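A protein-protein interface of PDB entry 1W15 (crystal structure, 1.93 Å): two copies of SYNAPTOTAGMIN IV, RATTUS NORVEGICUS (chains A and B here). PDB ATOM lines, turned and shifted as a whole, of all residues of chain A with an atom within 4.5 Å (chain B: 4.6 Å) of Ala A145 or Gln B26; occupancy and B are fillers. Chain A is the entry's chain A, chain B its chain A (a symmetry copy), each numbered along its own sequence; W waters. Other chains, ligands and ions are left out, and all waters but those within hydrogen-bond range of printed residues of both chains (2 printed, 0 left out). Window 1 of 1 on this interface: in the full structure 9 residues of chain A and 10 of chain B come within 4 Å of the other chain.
The side-chain hydroxyl of Thr B29 is in hydrogen-bond range of the side-chain hydroxyl of Thr B31.
OG of Ser A22 sits close to O of Ile A144, at 3.1 Å.
OG1 of Thr B29 lies close to O of Gln B26, at 3.4 Å.
The backbone NH of Gln B26 lies within hydrogen-bond range of the backbone carbonyl oxygen of Thr B31 (3.0 Å).
OE1 of Glu A135 lies within salt-bridge range of NZ of Lys A146, at 2.8 Å.
A ring nitrogen (NE2) of His A132 lies within hydrogen-bond range of the backbone carbonyl oxygen (O) of Ile A144.
Glu A135 touches Gln B26 (OE2 to NE2, 3.8 Å).
CG2 of Thr B29 touches OE2 of Glu A135, 3.9 Å away.
Ile A144 touches Gln B26.
Ala A145 touches Gln B26.
Printed residues of chain B within 4 Å of Glu A135: Gln B26 and Thr B29.
Of the printed residues of chain B, Ile A144 touches Gln B26.
Of the printed residues of chain A, Thr B29 touches Glu A135 (3.9 Å).
Asn B30 touches none of the printed residues of chain A.
The nearest printed residue of chain B that does not touch Ala A145 is Leu B85 (4.4 Å).
The nearest printed residue of chain A that does not touch Thr B29 is Lys A146 (4.8 Å).
Of the 9 printed residues of chain A, 3 touch a printed residue of chain B.
Printed residues of chain A that touch a printed residue of chain B: Glu A135, Ile A144 and Ala A145.
Hydrophobic or aromatic side chains of chain A within 4 Å of the printed part of chain B: Ile A144.
Of the 11 printed residues of chain B, 2 touch a printed residue of chain A.
Among the printed residues, 4 pairs touch across the chains.
No position is printed for both chains.
Of the 4 pairs that touch across the chains among the printed residues, none has its exchanged pair printed and touching as well.
Water W1 lies within hydrogen-bond range of the backbone carbonyl oxygen of Arg B141 and the backbone NH of Gln A143.
Water W2 lies within hydrogen-bond range of the backbone carbonyl oxygen (O) of Gln A143 (3.1 Å) and the side-chain sulfur (SG) of Cys B24 (3.6 Å).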
ATOM      1  N   VAL A  21     -27.124  -6.350  -7.786  1.00  0.00           N
ATOM      2  CA  VAL A  21     -27.697  -5.086  -7.297  1.00  0.00           C
ATOM      3  C   VAL A  21     -27.849  -5.192  -5.779  1.00  0.00           C
ATOM      4  O   VAL A  21     -27.926  -6.310  -5.258  1.00  0.00           O
ATOM      5  CB  VAL A  21     -29.054  -4.701  -7.945  1.00  0.00           C
ATOM      6  CG1 VAL A  21     -28.886  -4.402  -9.474  1.00  0.00           C
ATOM      7  CG2 VAL A  21     -30.162  -5.763  -7.660  1.00  0.00           C
ATOM      8  N   SER A  22     -27.765  -4.058  -5.087  1.00  0.00           N
ATOM      9  CA  SER A  22     -27.961  -4.072  -3.627  1.00  0.00           C
ATOM     10  C   SER A  22     -28.993  -3.011  -3.306  1.00  0.00           C
ATOM     11  O   SER A  22     -28.967  -1.922  -3.924  1.00  0.00           O
ATOM     12  CB  SER A  22     -26.627  -3.754  -2.904  1.00  0.00           C
ATOM     13  OG  SER A  22     -26.782  -3.818  -1.506  1.00  0.00           O
ATOM     14  N   LEU A  37     -24.250  -2.648  -9.126  1.00  0.00           N
ATOM     15  CA  LEU A  37     -22.887  -3.011  -8.796  1.00  0.00           C
ATOM     16  C   LEU A  37     -22.160  -3.441 -10.075  1.00  0.00           C
ATOM     17  O   LEU A  37     -21.211  -2.761 -10.489  1.00  0.00           O
ATOM     18  CB  LEU A  37     -22.851  -4.099  -7.721  1.00  0.00           C
ATOM     19  CG  LEU A  37     -23.264  -3.480  -6.368  1.00  0.00           C
ATOM     20  CD1 LEU A  37     -23.941  -4.461  -5.394  1.00  0.00           C
ATOM     21  CD2 LEU A  37     -21.962  -2.934  -5.730  1.00  0.00           C
ATOM     22  N   HIS A 132     -35.934 -11.066  -3.408  1.00  0.00           N
ATOM     23  CA  HIS A 132     -35.027  -9.988  -3.031  1.00  0.00           C
ATOM     24  C   HIS A 132     -35.868  -8.841  -2.437  1.00  0.00           C
ATOM     25  O   HIS A 132     -35.553  -8.321  -1.380  1.00  0.00           O
ATOM     26  CB  HIS A 132     -34.212  -9.518  -4.261  1.00  0.00           C
ATOM     27  CG  HIS A 132     -33.035  -8.643  -3.905  1.00  0.00           C
ATOM     28  ND1 HIS A 132     -32.083  -8.250  -4.833  1.00  0.00           N
ATOM     29  CD2 HIS A 132     -32.668  -8.068  -2.730  1.00  0.00           C
ATOM     30  CE1 HIS A 132     -31.176  -7.486  -4.245  1.00  0.00           C
ATOM     31  NE2 HIS A 132     -31.501  -7.363  -2.963  1.00  0.00           N
ATOM     32  N   GLU A 135     -37.149  -9.585   1.091  1.00  0.00           N
ATOM     33  CA  GLU A 135     -36.076  -9.518   2.075  1.00  0.00           C
ATOM     34  C   GLU A 135     -35.840  -8.040   2.453  1.00  0.00           C
ATOM     35  O   GLU A 135     -35.724  -7.715   3.649  1.00  0.00           O
ATOM     36  CB  GLU A 135     -34.807 -10.204   1.541  1.00  0.00           C
ATOM     37  CG  GLU A 135     -33.831 -10.625   2.635  1.00  0.00           C
ATOM     38  CD  GLU A 135     -32.621 -11.405   2.110  1.00  0.00           C
ATOM     39  OE1 GLU A 135     -32.709 -11.987   1.010  1.00  0.00           O
ATOM     40  OE2 GLU A 135     -31.580 -11.441   2.816  1.00  0.00           O
ATOM     41  N   GLN A 143     -28.611  -3.308   4.034  1.00  0.00           N
ATOM     42  CA  GLN A 143     -28.346  -3.318   2.588  1.00  0.00           C
ATOM     43  C   GLN A 143     -28.240  -4.772   2.234  1.00  0.00           C
ATOM     44  O   GLN A 143     -27.579  -5.524   2.943  1.00  0.00           O
ATOM     45  CB  GLN A 143     -27.032  -2.640   2.256  1.00  0.00           C
ATOM     46  CG  GLN A 143     -27.201  -1.281   1.684  1.00  0.00           C
ATOM     47  CD  GLN A 143     -26.997  -1.253   0.190  1.00  0.00           C
ATOM     48  OE1 GLN A 143     -27.882  -1.650  -0.564  1.00  0.00           O
ATOM     49  NE2 GLN A 143     -25.840  -0.726  -0.250  1.00  0.00           N
ATOM     50  N   ILE A 144     -28.949  -5.193   1.198  1.00  0.00           N
ATOM     51  CA  ILE A 144     -28.899  -6.592   0.798  1.00  0.00           C
ATOM     52  C   ILE A 144     -28.535  -6.616  -0.691  1.00  0.00           C
ATOM     53  O   ILE A 144     -29.134  -5.870  -1.466  1.00  0.00           O
ATOM     54  CB  ILE A 144     -30.261  -7.274   1.002  1.00  0.00           C
ATOM     55  CG1 ILE A 144     -30.763  -7.121   2.459  1.00  0.00           C
ATOM     56  CG2 ILE A 144     -30.213  -8.767   0.565  1.00  0.00           C
ATOM     57  CD1 ILE A 144     -32.303  -7.304   2.576  1.00  0.00           C
ATOM     58  N   ALA A 145     -27.578  -7.476  -1.044  1.00  0.00           N
ATOM     59  CA  ALA A 145     -27.046  -7.624  -2.450  1.00  0.00           C
ATOM     60  C   ALA A 145     -27.336  -9.006  -2.995  1.00  0.00           C
ATOM     61  O   ALA A 145     -27.202 -10.003  -2.240  1.00  0.00           O
ATOM     62  CB  ALA A 145     -25.557  -7.349  -2.487  1.00  0.00           C
ATOM     63  N   LYS A 146     -27.783  -9.108  -4.268  1.00  0.00           N
ATOM     64  CA  LYS A 146     -28.038 -10.412  -4.889  1.00  0.00           C
ATOM     65  C   LYS A 146     -27.754 -10.295  -6.377  1.00  0.00           C
ATOM     66  O   LYS A 146     -27.996  -9.226  -6.961  1.00  0.00           O
ATOM     67  CB  LYS A 146     -29.501 -10.881  -4.787  1.00  0.00           C
ATOM     68  CG  LYS A 146     -30.065 -10.948  -3.373  1.00  0.00           C
ATOM     69  CD  LYS A 146     -31.377 -11.819  -3.311  1.00  0.00           C
ATOM     70  CE  LYS A 146     -31.891 -11.899  -1.849  1.00  0.00           C
ATOM     71  NZ  LYS A 146     -30.758 -12.329  -0.942  1.00  0.00           N
ATOM     72  N   CYS B  24     -19.986  -9.013   5.192  1.00  0.00           N
ATOM     73  CA  CYS B  24     -21.339  -9.050   5.786  1.00  0.00           C
ATOM     74  C   CYS B  24     -21.853 -10.481   5.673  1.00  0.00           C
ATOM     75  O   CYS B  24     -21.905 -11.040   4.560  1.00  0.00           O
ATOM     76  CB  CYS B  24     -22.301  -8.123   5.026  1.00  0.00           C
ATOM     77  SG  CYS B  24     -23.944  -8.171   5.696  1.00  0.00           S
ATOM     78  N   TYR B  25     -22.234 -11.088   6.807  1.00  0.00           N
ATOM     79  CA  TYR B  25     -22.758 -12.453   6.810  1.00  0.00           C
ATOM     80  C   TYR B  25     -24.300 -12.382   6.871  1.00  0.00           C
ATOM     81  O   TYR B  25     -24.885 -11.901   7.841  1.00  0.00           O
ATOM     82  CB  TYR B  25     -22.235 -13.237   8.019  1.00  0.00           C
ATOM     83  CG  TYR B  25     -22.783 -14.650   8.180  1.00  0.00           C
ATOM     84  CD1 TYR B  25     -22.951 -15.487   7.074  1.00  0.00           C
ATOM     85  CD2 TYR B  25     -23.107 -15.167   9.461  1.00  0.00           C
ATOM     86  CE1 TYR B  25     -23.442 -16.802   7.209  1.00  0.00           C
ATOM     87  CE2 TYR B  25     -23.585 -16.493   9.607  1.00  0.00           C
ATOM     88  CZ  TYR B  25     -23.753 -17.288   8.475  1.00  0.00           C
ATOM     89  OH  TYR B  25     -24.232 -18.579   8.565  1.00  0.00           O
ATOM     90  N   GLN B  26     -24.914 -12.810   5.778  1.00  0.00           N
ATOM     91  CA  GLN B  26     -26.372 -12.874   5.631  1.00  0.00           C
ATOM     92  C   GLN B  26     -26.783 -14.239   6.270  1.00  0.00           C
ATOM     93  O   GLN B  26     -27.027 -15.212   5.550  1.00  0.00           O
ATOM     94  CB  GLN B  26     -26.780 -12.637   4.102  1.00  0.00           C
ATOM     95  CG  GLN B  26     -26.018 -11.561   3.293  1.00  0.00           C
ATOM     96  CD  GLN B  26     -26.758 -10.844   2.149  1.00  0.00           C
ATOM     97  OE1 GLN B  26     -26.181  -9.952   1.519  1.00  0.00           O
ATOM     98  NE2 GLN B  26     -28.005 -11.053   1.745  1.00  0.00           N
ATOM     99  N   SER B  27     -26.847 -14.276   7.622  1.00  0.00           N
ATOM    100  CA  SER B  27     -27.056 -15.557   8.327  1.00  0.00           C
ATOM    101  C   SER B  27     -28.300 -16.369   7.927  1.00  0.00           C
ATOM    102  O   SER B  27     -28.242 -17.616   7.898  1.00  0.00           O
ATOM    103  CB  SER B  27     -27.019 -15.392   9.865  1.00  0.00           C
ATOM    104  OG  SER B  27     -28.185 -14.773  10.372  1.00  0.00           O
ATOM    105  N   THR B  28     -29.420 -15.691   7.646  1.00  0.00           N
ATOM    106  CA  THR B  28     -30.669 -16.412   7.279  1.00  0.00           C
ATOM    107  C   THR B  28     -30.628 -16.946   5.846  1.00  0.00           C
ATOM    108  O   THR B  28     -31.441 -17.796   5.483  1.00  0.00           O
ATOM    109  CB  THR B  28     -31.932 -15.537   7.433  1.00  0.00           C
ATOM    110  OG1 THR B  28     -31.855 -14.415   6.535  1.00  0.00           O
ATOM    111  CG2 THR B  28     -32.006 -14.922   8.801  1.00  0.00           C
ATOM    112  N   THR B  29     -29.699 -16.455   5.031  1.00  0.00           N
ATOM    113  CA  THR B  29     -29.614 -16.965   3.627  1.00  0.00           C
ATOM    114  C   THR B  29     -28.285 -17.634   3.234  1.00  0.00           C
ATOM    115  O   THR B  29     -28.086 -17.973   2.081  1.00  0.00           O
ATOM    116  CB  THR B  29     -29.901 -15.923   2.617  1.00  0.00           C
ATOM    117  OG1 THR B  29     -28.968 -14.830   2.791  1.00  0.00           O
ATOM    118  CG2 THR B  29     -31.306 -15.364   2.826  1.00  0.00           C
ATOM    119  N   ASN B  30     -27.411 -17.844   4.200  1.00  0.00           N
ATOM    120  CA  ASN B  30     -26.141 -18.515   3.925  1.00  0.00           C
ATOM    121  C   ASN B  30     -25.395 -17.892   2.747  1.00  0.00           C
ATOM    122  O   ASN B  30     -25.004 -18.602   1.817  1.00  0.00           O
ATOM    123  CB  ASN B  30     -26.427 -19.985   3.624  1.00  0.00           C
ATOM    124  CG  ASN B  30     -27.416 -20.561   4.588  1.00  0.00           C
ATOM    125  OD1 ASN B  30     -27.205 -20.539   5.833  1.00  0.00           O
ATOM    126  ND2 ASN B  30     -28.525 -21.062   4.042  1.00  0.00           N
ATOM    127  N   THR B  31     -25.257 -16.572   2.743  1.00  0.00           N
ATOM    128  CA  THR B  31     -24.340 -15.932   1.775  1.00  0.00           C
ATOM    129  C   THR B  31     -23.437 -15.045   2.573  1.00  0.00           C
ATOM    130  O   THR B  31     -23.772 -14.641   3.697  1.00  0.00           O
ATOM    131  CB  THR B  31     -25.009 -15.083   0.655  1.00  0.00           C
ATOM    132  OG1 THR B  31     -26.004 -14.262   1.226  1.00  0.00           O
ATOM    133  CG2 THR B  31     -25.733 -15.939  -0.442  1.00  0.00           C
ATOM    134  N   THR B  33     -21.029 -11.629   1.878  1.00  0.00           N
ATOM    135  CA  THR B  33     -20.595 -10.672   0.869  1.00  0.00           C
ATOM    136  C   THR B  33     -19.257 -10.104   1.298  1.00  0.00           C
ATOM    137  O   THR B  33     -19.041  -9.792   2.476  1.00  0.00           O
ATOM    138  CB  THR B  33     -21.672  -9.596   0.622  1.00  0.00           C
ATOM    139  OG1 THR B  33     -21.639  -8.624   1.663  1.00  0.00           O
ATOM    140  CG2 THR B  33     -23.067 -10.254   0.770  1.00  0.00           C
ATOM    141  N   LEU B  85     -17.213  -5.845  -5.033  1.00  0.00           N
ATOM    142  CA  LEU B  85     -18.040  -6.676  -4.137  1.00  0.00           C
ATOM    143  C   LEU B  85     -18.244  -8.055  -4.773  1.00  0.00           C
ATOM    144  O   LEU B  85     -18.575  -8.177  -5.997  1.00  0.00           O
ATOM    145  CB  LEU B  85     -19.362  -5.997  -3.829  1.00  0.00           C
ATOM    146  CG  LEU B  85     -20.355  -6.704  -2.864  1.00  0.00           C
ATOM    147  CD1 LEU B  85     -21.187  -5.578  -2.146  1.00  0.00           C
ATOM    148  CD2 LEU B  85     -21.272  -7.699  -3.595  1.00  0.00           C
ATOM    149  N   ARG B 141     -25.684  -9.691   9.136  1.00  0.00           N
ATOM    150  CA  ARG B 141     -26.377  -8.622   8.374  1.00  0.00           C
ATOM    151  C   ARG B 141     -25.779  -7.234   8.523  1.00  0.00           C
ATOM    152  O   ARG B 141     -26.303  -6.287   7.927  1.00  0.00           O
ATOM    153  CB  ARG B 141     -27.918  -8.579   8.646  1.00  0.00           C
ATOM    154  CG  ARG B 141     -28.664  -9.766   8.069  1.00  0.00           C
ATOM    155  CD  ARG B 141     -30.171  -9.948   8.585  1.00  0.00           C
ATOM    156  NE  ARG B 141     -30.156 -10.124  10.042  1.00  0.00           N
ATOM    157  CZ  ARG B 141     -29.852 -11.247  10.651  1.00  0.00           C
ATOM    158  NH1 ARG B 141     -29.596 -12.336   9.958  1.00  0.00           N
ATOM    159  NH2 ARG B 141     -29.742 -11.270  11.947  1.00  0.00           N
HETATM  160  O   HOH W   1     -26.365  -4.057   6.050  1.00  0.00           O
HETATM  161  O   HOH W   2     -27.439  -7.973   4.809  1.00  0.00           O
